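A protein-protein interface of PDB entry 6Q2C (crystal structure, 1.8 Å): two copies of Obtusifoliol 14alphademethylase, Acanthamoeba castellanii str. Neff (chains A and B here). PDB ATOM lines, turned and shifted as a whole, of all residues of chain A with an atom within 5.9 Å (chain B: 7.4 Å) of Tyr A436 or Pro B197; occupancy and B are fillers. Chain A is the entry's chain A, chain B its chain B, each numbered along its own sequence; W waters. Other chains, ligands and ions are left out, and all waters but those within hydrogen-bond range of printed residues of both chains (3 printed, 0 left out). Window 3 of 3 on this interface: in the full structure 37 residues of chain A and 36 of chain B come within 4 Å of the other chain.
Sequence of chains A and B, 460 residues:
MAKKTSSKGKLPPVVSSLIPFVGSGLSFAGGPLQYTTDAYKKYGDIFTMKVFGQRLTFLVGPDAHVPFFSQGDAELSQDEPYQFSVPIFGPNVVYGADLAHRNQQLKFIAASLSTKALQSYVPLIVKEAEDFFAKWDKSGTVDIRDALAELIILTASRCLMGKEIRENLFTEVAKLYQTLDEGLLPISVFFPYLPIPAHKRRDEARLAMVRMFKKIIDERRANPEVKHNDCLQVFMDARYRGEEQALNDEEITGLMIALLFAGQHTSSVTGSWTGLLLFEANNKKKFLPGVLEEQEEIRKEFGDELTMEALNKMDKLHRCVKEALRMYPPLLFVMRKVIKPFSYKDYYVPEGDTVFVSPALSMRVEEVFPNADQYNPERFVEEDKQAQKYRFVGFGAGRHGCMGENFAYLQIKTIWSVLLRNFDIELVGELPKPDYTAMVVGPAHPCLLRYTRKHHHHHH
Hydrophobic or aromatic side chains of chain A within 4 Å of the printed part of chain B: Tyr A436. Hydrophobic or aromatic side chains of chain B within 4 Å of the printed part of chain A: Leu B194, Ile B196 and Pro B197. Among the printed residues, no Asp or Glu carboxylate lies within 4 Å of a Lys or Arg side-chain nitrogen of the other chain.
Water W1 lies within hydrogen-bond range of the backbone carbonyl oxygen (O) of Pro A434 (2.7 Å) and the guanidinium group (NH1) of Arg B201 (3.1 Å). Water W2 lies within hydrogen-bond range of O of Gly A30 (2.7 Å) and N of Ala B198 (2.9 Å). Water W3 lies within hydrogen-bond range of the backbone carbonyl oxygen (O) of Pro A434 and the guanidinium group (NH2) of Arg B201.
The backbone carbonyl oxygen (O) of Leu B194 sits at hydrogen-bond distance from a ring nitrogen (ND1) of His B199, 2.8 Å away.
No position is printed for both chains. Of the 8 pairs that touch across the chains among the printed residues, none has its exchanged pair printed and touching as well.
Among the printed residues, merely in contact across the chains: Gly A30 with Ile B196 (3.4 Å), Ala A29 with Ile B196 (3.5 Å), Gly A30 with Pro B197 (3.7 Å), Gly A31 with Pro B197 (3.7 Å), Ala A29 with Leu B194 (3.7 Å), Pro A32 with Ile B196 (3.7 Å), Gly A31 with Ile B196 (3.8 Å) and Tyr A436 with Pro B197 (3.9 Å).
Pro B197 touches three residues of chain A. Of the printed residues of chain B, Gly A31 touches Ile B196 and Pro B197. Printed residues of chain A within 4 Å of Ile B196: Ala A29 (3.5 Å), Gly A30 (3.4 Å), Gly A31 (3.8 Å) and Pro A32 (3.7 Å). Printed residues of chain B within 4 Å of Gly A30: Ile B196 and Pro B197. Of the printed residues of chain A, Leu B194 touches Ala A29. The nearest residue of chain B that does not touch Tyr A436 is Leu B185 (6.0 Å). The nearest printed residue of chain B that does not touch Pro A32 is Leu B194 (4.4 Å).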
ATOM      1  N   SER A  27      -5.461  23.667 -32.337  1.00  0.00           N
ATOM      2  CA  SER A  27      -5.986  22.741 -33.362  1.00  0.00           C
ATOM      3  C   SER A  27      -4.969  21.701 -33.906  1.00  0.00           C
ATOM      4  O   SER A  27      -5.342  20.652 -34.495  1.00  0.00           O
ATOM      5  CB  SER A  27      -6.697  23.561 -34.451  1.00  0.00           C
ATOM      6  OG  SER A  27      -7.831  24.170 -33.750  1.00  0.00           O
ATOM      7  N   PHE A  28      -3.694  22.000 -33.689  1.00  0.00           N
ATOM      8  CA  PHE A  28      -2.607  21.171 -34.097  1.00  0.00           C
ATOM      9  C   PHE A  28      -1.770  20.759 -32.947  1.00  0.00           C
ATOM     10  O   PHE A  28      -0.578  20.568 -33.077  1.00  0.00           O
ATOM     11  CB  PHE A  28      -1.753  21.964 -35.110  1.00  0.00           C
ATOM     12  CG  PHE A  28      -2.334  22.014 -36.479  1.00  0.00           C
ATOM     13  CD1 PHE A  28      -2.397  20.854 -37.254  1.00  0.00           C
ATOM     14  CD2 PHE A  28      -2.893  23.160 -36.982  1.00  0.00           C
ATOM     15  CE1 PHE A  28      -2.918  20.862 -38.534  1.00  0.00           C
ATOM     16  CE2 PHE A  28      -3.401  23.162 -38.256  1.00  0.00           C
ATOM     17  CZ  PHE A  28      -3.402  22.036 -39.040  1.00  0.00           C
ATOM     18  N   ALA A  29      -2.339  20.613 -31.764  1.00  0.00           N
ATOM     19  CA  ALA A  29      -1.565  20.246 -30.627  1.00  0.00           C
ATOM     20  C   ALA A  29      -1.651  18.731 -30.269  1.00  0.00           C
ATOM     21  O   ALA A  29      -1.376  18.325 -29.080  1.00  0.00           O
ATOM     22  CB  ALA A  29      -2.020  21.074 -29.450  1.00  0.00           C
ATOM     23  N   GLY A  30      -2.102  17.911 -31.229  1.00  0.00           N
ATOM     24  CA  GLY A  30      -2.128  16.450 -31.102  1.00  0.00           C
ATOM     25  C   GLY A  30      -3.247  15.934 -30.176  1.00  0.00           C
ATOM     26  O   GLY A  30      -3.157  14.808 -29.645  1.00  0.00           O
ATOM     27  N   GLY A  31      -4.277  16.755 -29.979  1.00  0.00           N
ATOM     28  CA  GLY A  31      -5.427  16.299 -29.175  1.00  0.00           C
ATOM     29  C   GLY A  31      -5.278  16.289 -27.661  1.00  0.00           C
ATOM     30  O   GLY A  31      -5.540  15.256 -27.023  1.00  0.00           O
ATOM     31  N   PRO A  32      -4.987  17.455 -27.041  1.00  0.00           N
ATOM     32  CA  PRO A  32      -4.745  17.539 -25.578  1.00  0.00           C
ATOM     33  C   PRO A  32      -6.059  17.546 -24.765  1.00  0.00           C
ATOM     34  O   PRO A  32      -6.240  18.373 -23.825  1.00  0.00           O
ATOM     35  CB  PRO A  32      -3.978  18.867 -25.416  1.00  0.00           C
ATOM     36  CG  PRO A  32      -4.609  19.687 -26.505  1.00  0.00           C
ATOM     37  CD  PRO A  32      -4.834  18.762 -27.675  1.00  0.00           C
ATOM     38  N   LEU A  33      -6.917  16.582 -25.074  1.00  0.00           N
ATOM     39  CA  LEU A  33      -8.200  16.420 -24.344  1.00  0.00           C
ATOM     40  C   LEU A  33      -8.048  16.046 -22.898  1.00  0.00           C
ATOM     41  O   LEU A  33      -8.750  16.621 -22.017  1.00  0.00           O
ATOM     42  CB  LEU A  33      -9.078  15.403 -25.041  1.00  0.00           C
ATOM     43  CG  LEU A  33      -9.653  15.869 -26.378  1.00  0.00           C
ATOM     44  CD1 LEU A  33     -10.651  14.820 -26.888  1.00  0.00           C
ATOM     45  CD2 LEU A  33     -10.335  17.264 -26.239  1.00  0.00           C
ATOM     46  N   LEU A 332     -12.340  20.018 -32.170  1.00  0.00           N
ATOM     47  CA  LEU A 332     -12.171  19.875 -30.749  1.00  0.00           C
ATOM     48  C   LEU A 332     -12.383  21.176 -29.996  1.00  0.00           C
ATOM     49  O   LEU A 332     -12.788  21.101 -28.820  1.00  0.00           O
ATOM     50  CB  LEU A 332     -10.762  19.444 -30.440  1.00  0.00           C
ATOM     51  CG  LEU A 332     -10.474  18.039 -30.944  1.00  0.00           C
ATOM     52  CD1 LEU A 332      -9.140  17.718 -30.277  1.00  0.00           C
ATOM     53  CD2 LEU A 332     -11.626  17.041 -30.652  1.00  0.00           C
ATOM     54  N   PRO A 434      -9.339   8.071 -32.157  1.00  0.00           N
ATOM     55  CA  PRO A 434      -9.281   9.309 -32.897  1.00  0.00           C
ATOM     56  C   PRO A 434      -7.866   9.566 -33.400  1.00  0.00           C
ATOM     57  O   PRO A 434      -6.877   9.145 -32.782  1.00  0.00           O
ATOM     58  CB  PRO A 434      -9.700  10.373 -31.866  1.00  0.00           C
ATOM     59  CG  PRO A 434     -10.452   9.641 -30.840  1.00  0.00           C
ATOM     60  CD  PRO A 434      -9.882   8.261 -30.801  1.00  0.00           C
ATOM     61  N   ASP A 435      -7.797  10.199 -34.545  1.00  0.00           N
ATOM     62  CA  ASP A 435      -6.526  10.614 -35.187  1.00  0.00           C
ATOM     63  C   ASP A 435      -6.443  12.119 -35.113  1.00  0.00           C
ATOM     64  O   ASP A 435      -7.237  12.839 -35.701  1.00  0.00           O
ATOM     65  CB  ASP A 435      -6.571  10.134 -36.608  1.00  0.00           C
ATOM     66  CG  ASP A 435      -5.551  10.763 -37.555  1.00  0.00           C
ATOM     67  OD1 ASP A 435      -4.668  11.544 -37.201  1.00  0.00           O
ATOM     68  OD2 ASP A 435      -5.701  10.397 -38.751  1.00  0.00           O
ATOM     69  N   TYR A 436      -5.465  12.597 -34.393  1.00  0.00           N
ATOM     70  CA  TYR A 436      -5.323  14.052 -34.171  1.00  0.00           C
ATOM     71  C   TYR A 436      -4.264  14.726 -35.027  1.00  0.00           C
ATOM     72  O   TYR A 436      -3.790  15.786 -34.642  1.00  0.00           O
ATOM     73  CB  TYR A 436      -5.067  14.356 -32.683  1.00  0.00           C
ATOM     74  CG  TYR A 436      -6.129  13.865 -31.740  1.00  0.00           C
ATOM     75  CD1 TYR A 436      -7.293  14.576 -31.606  1.00  0.00           C
ATOM     76  CD2 TYR A 436      -5.967  12.729 -30.950  1.00  0.00           C
ATOM     77  CE1 TYR A 436      -8.328  14.133 -30.763  1.00  0.00           C
ATOM     78  CE2 TYR A 436      -7.003  12.276 -30.105  1.00  0.00           C
ATOM     79  CZ  TYR A 436      -8.173  13.014 -30.019  1.00  0.00           C
ATOM     80  OH  TYR A 436      -9.237  12.741 -29.201  1.00  0.00           O
ATOM     81  N   THR A 437      -3.956  14.206 -36.211  1.00  0.00           N
ATOM     82  CA  THR A 437      -2.932  14.827 -37.066  1.00  0.00           C
ATOM     83  C   THR A 437      -3.421  15.951 -37.996  1.00  0.00           C
ATOM     84  O   THR A 437      -2.597  16.597 -38.657  1.00  0.00           O
ATOM     85  CB  THR A 437      -2.228  13.749 -37.905  1.00  0.00           C
ATOM     86  OG1 THR A 437      -3.169  13.146 -38.813  1.00  0.00           O
ATOM     87  CG2 THR A 437      -1.606  12.691 -36.962  1.00  0.00           C
ATOM     88  N   ALA A 438      -4.737  16.153 -38.109  1.00  0.00           N
ATOM     89  CA  ALA A 438      -5.257  17.281 -38.884  1.00  0.00           C
ATOM     90  C   ALA A 438      -6.193  18.104 -38.014  1.00  0.00           C
ATOM     91  O   ALA A 438      -6.596  17.702 -36.907  1.00  0.00           O
ATOM     92  CB  ALA A 438      -5.945  16.804 -40.169  1.00  0.00           C
ATOM     93  N   MET A 439      -6.476  19.280 -38.497  1.00  0.00           N
ATOM     94  CA  MET A 439      -7.342  20.198 -37.830  1.00  0.00           C
ATOM     95  C   MET A 439      -8.712  19.547 -37.516  1.00  0.00           C
ATOM     96  O   MET A 439      -9.257  19.841 -36.461  1.00  0.00           O
ATOM     97  CB  MET A 439      -7.551  21.418 -38.718  1.00  0.00           C
ATOM     98  CG  MET A 439      -8.435  22.464 -38.045  1.00  0.00           C
ATOM     99  SD  MET A 439      -8.647  24.026 -38.954  1.00  0.00           S
ATOM    100  CE  MET A 439      -6.980  24.623 -38.559  1.00  0.00           C
ATOM    101  N   VAL A 441     -10.586  16.168 -36.611  1.00  0.00           N
ATOM    102  CA  VAL A 441     -10.279  14.888 -36.039  1.00  0.00           C
ATOM    103  C   VAL A 441     -11.230  13.828 -36.604  1.00  0.00           C
ATOM    104  O   VAL A 441     -12.436  14.045 -36.756  1.00  0.00           O
ATOM    105  CB  VAL A 441     -10.504  14.974 -34.523  1.00  0.00           C
ATOM    106  CG1 VAL A 441     -10.268  13.662 -33.813  1.00  0.00           C
ATOM    107  CG2 VAL A 441      -9.670  16.103 -33.944  1.00  0.00           C
ATOM    108  N   GLY A 442     -10.692  12.679 -36.949  1.00  0.00           N
ATOM    109  CA  GLY A 442     -11.508  11.558 -37.454  1.00  0.00           C
ATOM    110  C   GLY A 442     -10.980  10.240 -36.927  1.00  0.00           C
ATOM    111  O   GLY A 442      -9.997  10.210 -36.215  1.00  0.00           O
ATOM    112  N   THR B 179       5.830   3.053 -33.569  1.00  0.00           N
ATOM    113  CA  THR B 179       5.071   3.769 -32.581  1.00  0.00           C
ATOM    114  C   THR B 179       5.898   4.914 -31.918  1.00  0.00           C
ATOM    115  O   THR B 179       5.365   5.993 -31.659  1.00  0.00           O
ATOM    116  CB  THR B 179       4.578   2.761 -31.531  1.00  0.00           C
ATOM    117  OG1 THR B 179       3.905   1.705 -32.193  1.00  0.00           O
ATOM    118  CG2 THR B 179       3.630   3.370 -30.563  1.00  0.00           C
ATOM    119  N   GLY B 183       5.181   9.109 -32.403  1.00  0.00           N
ATOM    120  CA  GLY B 183       5.178   9.977 -31.268  1.00  0.00           C
ATOM    121  C   GLY B 183       5.844  11.320 -31.471  1.00  0.00           C
ATOM    122  O   GLY B 183       5.737  12.174 -30.621  1.00  0.00           O
ATOM    123  N   LEU B 185       5.749  14.535 -33.052  1.00  0.00           N
ATOM    124  CA  LEU B 185       4.888  15.448 -33.835  1.00  0.00           C
ATOM    125  C   LEU B 185       5.377  16.883 -33.728  1.00  0.00           C
ATOM    126  O   LEU B 185       6.186  17.204 -32.877  1.00  0.00           O
ATOM    127  CB  LEU B 185       3.478  15.371 -33.203  1.00  0.00           C
ATOM    128  CG  LEU B 185       2.826  13.944 -33.258  1.00  0.00           C
ATOM    129  CD1 LEU B 185       1.519  13.905 -32.459  1.00  0.00           C
ATOM    130  CD2 LEU B 185       2.530  13.549 -34.687  1.00  0.00           C
ATOM    131  N   LEU B 194       3.775  16.571 -22.973  1.00  0.00           N
ATOM    132  CA  LEU B 194       2.332  16.860 -23.060  1.00  0.00           C
ATOM    133  C   LEU B 194       1.580  15.534 -23.107  1.00  0.00           C
ATOM    134  O   LEU B 194       1.905  14.663 -23.909  1.00  0.00           O
ATOM    135  CB  LEU B 194       2.020  17.690 -24.309  1.00  0.00           C
ATOM    136  CG  LEU B 194       0.590  18.240 -24.422  1.00  0.00           C
ATOM    137  CD1 LEU B 194       0.284  19.307 -23.341  1.00  0.00           C
ATOM    138  CD2 LEU B 194       0.356  18.821 -25.821  1.00  0.00           C
ATOM    139  N   PRO B 195       0.611  15.341 -22.208  1.00  0.00           N
ATOM    140  CA  PRO B 195       0.019  13.980 -22.180  1.00  0.00           C
ATOM    141  C   PRO B 195      -1.042  13.734 -23.234  1.00  0.00           C
ATOM    142  O   PRO B 195      -2.144  13.425 -22.892  1.00  0.00           O
ATOM    143  CB  PRO B 195      -0.563  13.892 -20.730  1.00  0.00           C
ATOM    144  CG  PRO B 195      -0.983  15.306 -20.433  1.00  0.00           C
ATOM    145  CD  PRO B 195       0.161  16.143 -21.050  1.00  0.00           C
ATOM    146  N   ILE B 196      -0.669  13.775 -24.508  1.00  0.00           N
ATOM    147  CA  ILE B 196      -1.551  13.489 -25.662  1.00  0.00           C
ATOM    148  C   ILE B 196      -1.424  12.048 -26.002  1.00  0.00           C
ATOM    149  O   ILE B 196      -0.392  11.403 -25.627  1.00  0.00           O
ATOM    150  CB  ILE B 196      -1.197  14.302 -26.899  1.00  0.00           C
ATOM    151  CG1 ILE B 196       0.350  14.228 -27.194  1.00  0.00           C
ATOM    152  CG2 ILE B 196      -1.650  15.772 -26.687  1.00  0.00           C
ATOM    153  CD1 ILE B 196       0.758  14.782 -28.544  1.00  0.00           C
ATOM    154  N   PRO B 197      -2.396  11.517 -26.746  1.00  0.00           N
ATOM    155  CA  PRO B 197      -2.361  10.081 -27.025  1.00  0.00           C
ATOM    156  C   PRO B 197      -1.099   9.567 -27.724  1.00  0.00           C
ATOM    157  O   PRO B 197      -0.622   8.458 -27.416  1.00  0.00           O
ATOM    158  CB  PRO B 197      -3.581   9.878 -27.942  1.00  0.00           C
ATOM    159  CG  PRO B 197      -4.549  10.885 -27.390  1.00  0.00           C
ATOM    160  CD  PRO B 197      -3.667  12.095 -27.251  1.00  0.00           C
ATOM    161  N   ALA B 198      -0.587  10.289 -28.704  1.00  0.00           N
ATOM    162  CA  ALA B 198       0.639   9.807 -29.403  1.00  0.00           C
ATOM    163  C   ALA B 198       1.868   9.755 -28.449  1.00  0.00           C
ATOM    164  O   ALA B 198       2.753   8.901 -28.623  1.00  0.00           O
ATOM    165  CB  ALA B 198       0.909  10.673 -30.618  1.00  0.00           C
ATOM    166  N   HIS B 199       1.925  10.629 -27.442  1.00  0.00           N
ATOM    167  CA  HIS B 199       2.972  10.560 -26.450  1.00  0.00           C
ATOM    168  C   HIS B 199       2.792   9.367 -25.486  1.00  0.00           C
ATOM    169  O   HIS B 199       3.750   8.726 -25.090  1.00  0.00           O
ATOM    170  CB  HIS B 199       3.071  11.830 -25.650  1.00  0.00           C
ATOM    171  CG  HIS B 199       3.646  12.977 -26.442  1.00  0.00           C
ATOM    172  ND1 HIS B 199       3.715  14.261 -25.953  1.00  0.00           N
ATOM    173  CD2 HIS B 199       4.192  13.007 -27.676  1.00  0.00           C
ATOM    174  CE1 HIS B 199       4.276  15.042 -26.868  1.00  0.00           C
ATOM    175  NE2 HIS B 199       4.549  14.306 -27.928  1.00  0.00           N
ATOM    176  N   LYS B 200       1.567   9.147 -25.069  1.00  0.00           N
ATOM    177  CA  LYS B 200       1.288   8.018 -24.211  1.00  0.00           C
ATOM    178  C   LYS B 200       1.675   6.701 -24.887  1.00  0.00           C
ATOM    179  O   LYS B 200       2.278   5.851 -24.245  1.00  0.00           O
ATOM    180  CB  LYS B 200      -0.184   7.985 -23.814  1.00  0.00           C
ATOM    181  CG  LYS B 200      -0.587   9.123 -22.902  1.00  0.00           C
ATOM    182  CD  LYS B 200      -1.930   8.795 -22.217  1.00  0.00           C
ATOM    183  CE  LYS B 200      -2.291   9.926 -21.296  1.00  0.00           C
ATOM    184  N   ARG B 201       1.351   6.567 -26.173  1.00  0.00           N
ATOM    185  CA  ARG B 201       1.716   5.416 -26.974  1.00  0.00           C
ATOM    186  C   ARG B 201       3.248   5.297 -27.198  1.00  0.00           C
ATOM    187  O   ARG B 201       3.800   4.208 -27.126  1.00  0.00           O
ATOM    188  CB  ARG B 201       0.928   5.366 -28.269  1.00  0.00           C
ATOM    189  CG  ARG B 201      -0.586   5.035 -28.061  1.00  0.00           C
ATOM    190  CD  ARG B 201      -1.321   4.782 -29.361  1.00  0.00           C
ATOM    191  NE  ARG B 201      -1.341   5.990 -30.167  1.00  0.00           N
ATOM    192  CZ  ARG B 201      -2.409   6.800 -30.444  1.00  0.00           C
ATOM    193  NH1 ARG B 201      -3.693   6.576 -30.045  1.00  0.00           N
ATOM    194  NH2 ARG B 201      -2.174   7.880 -31.197  1.00  0.00           N
ATOM    195  N   ARG B 202       3.929   6.422 -27.378  1.00  0.00           N
ATOM    196  CA  ARG B 202       5.430   6.449 -27.398  1.00  0.00           C
ATOM    197  C   ARG B 202       6.010   5.882 -26.096  1.00  0.00           C
ATOM    198  O   ARG B 202       6.927   5.035 -26.106  1.00  0.00           O
ATOM    199  CB  ARG B 202       5.937   7.888 -27.666  1.00  0.00           C
ATOM    200  CG  ARG B 202       7.418   8.225 -27.409  1.00  0.00           C
ATOM    201  CD  ARG B 202       7.583   9.720 -27.218  1.00  0.00           C
ATOM    202  NE  ARG B 202       7.047  10.154 -25.925  1.00  0.00           N
ATOM    203  CZ  ARG B 202       6.863  11.417 -25.527  1.00  0.00           C
ATOM    204  NH1 ARG B 202       7.219  12.484 -26.271  1.00  0.00           N
ATOM    205  NH2 ARG B 202       6.348  11.630 -24.341  1.00  0.00           N
ATOM    206  N   ASP B 203       5.508   6.355 -24.973  1.00  0.00           N
ATOM    207  CA  ASP B 203       6.078   5.951 -23.702  1.00  0.00           C
ATOM    208  C   ASP B 203       5.870   4.429 -23.472  1.00  0.00           C
ATOM    209  O   ASP B 203       6.776   3.742 -23.014  1.00  0.00           O
ATOM    210  CB  ASP B 203       5.521   6.754 -22.510  1.00  0.00           C
ATOM    211  CG  ASP B 203       5.862   8.259 -22.576  1.00  0.00           C
ATOM    212  OD1 ASP B 203       6.704   8.697 -23.431  1.00  0.00           O
ATOM    213  OD2 ASP B 203       5.221   9.008 -21.817  1.00  0.00           O
ATOM    214  N   GLU B 204       4.702   3.935 -23.852  1.00  0.00           N
ATOM    215  CA  GLU B 204       4.380   2.494 -23.734  1.00  0.00           C
ATOM    216  C   GLU B 204       5.354   1.687 -24.588  1.00  0.00           C
ATOM    217  O   GLU B 204       5.930   0.737 -24.086  1.00  0.00           O
ATOM    218  CB  GLU B 204       2.963   2.190 -24.252  1.00  0.00           C
ATOM    219  CG  GLU B 204       1.811   2.496 -23.301  1.00  0.00           C
ATOM    220  CD  GLU B 204       0.429   2.576 -24.022  1.00  0.00           C
ATOM    221  OE1 GLU B 204      -0.496   3.248 -23.496  1.00  0.00           O
ATOM    222  OE2 GLU B 204       0.263   2.009 -25.139  1.00  0.00           O
HETATM  223  O   HOH W   1      -5.808   8.765 -30.385  1.00  0.00           O
HETATM  224  O   HOH W   2      -1.860  12.466 -30.221  1.00  0.00           O
HETATM  225  O   HOH W   3      -4.543   7.531 -33.487  1.00  0.00           O
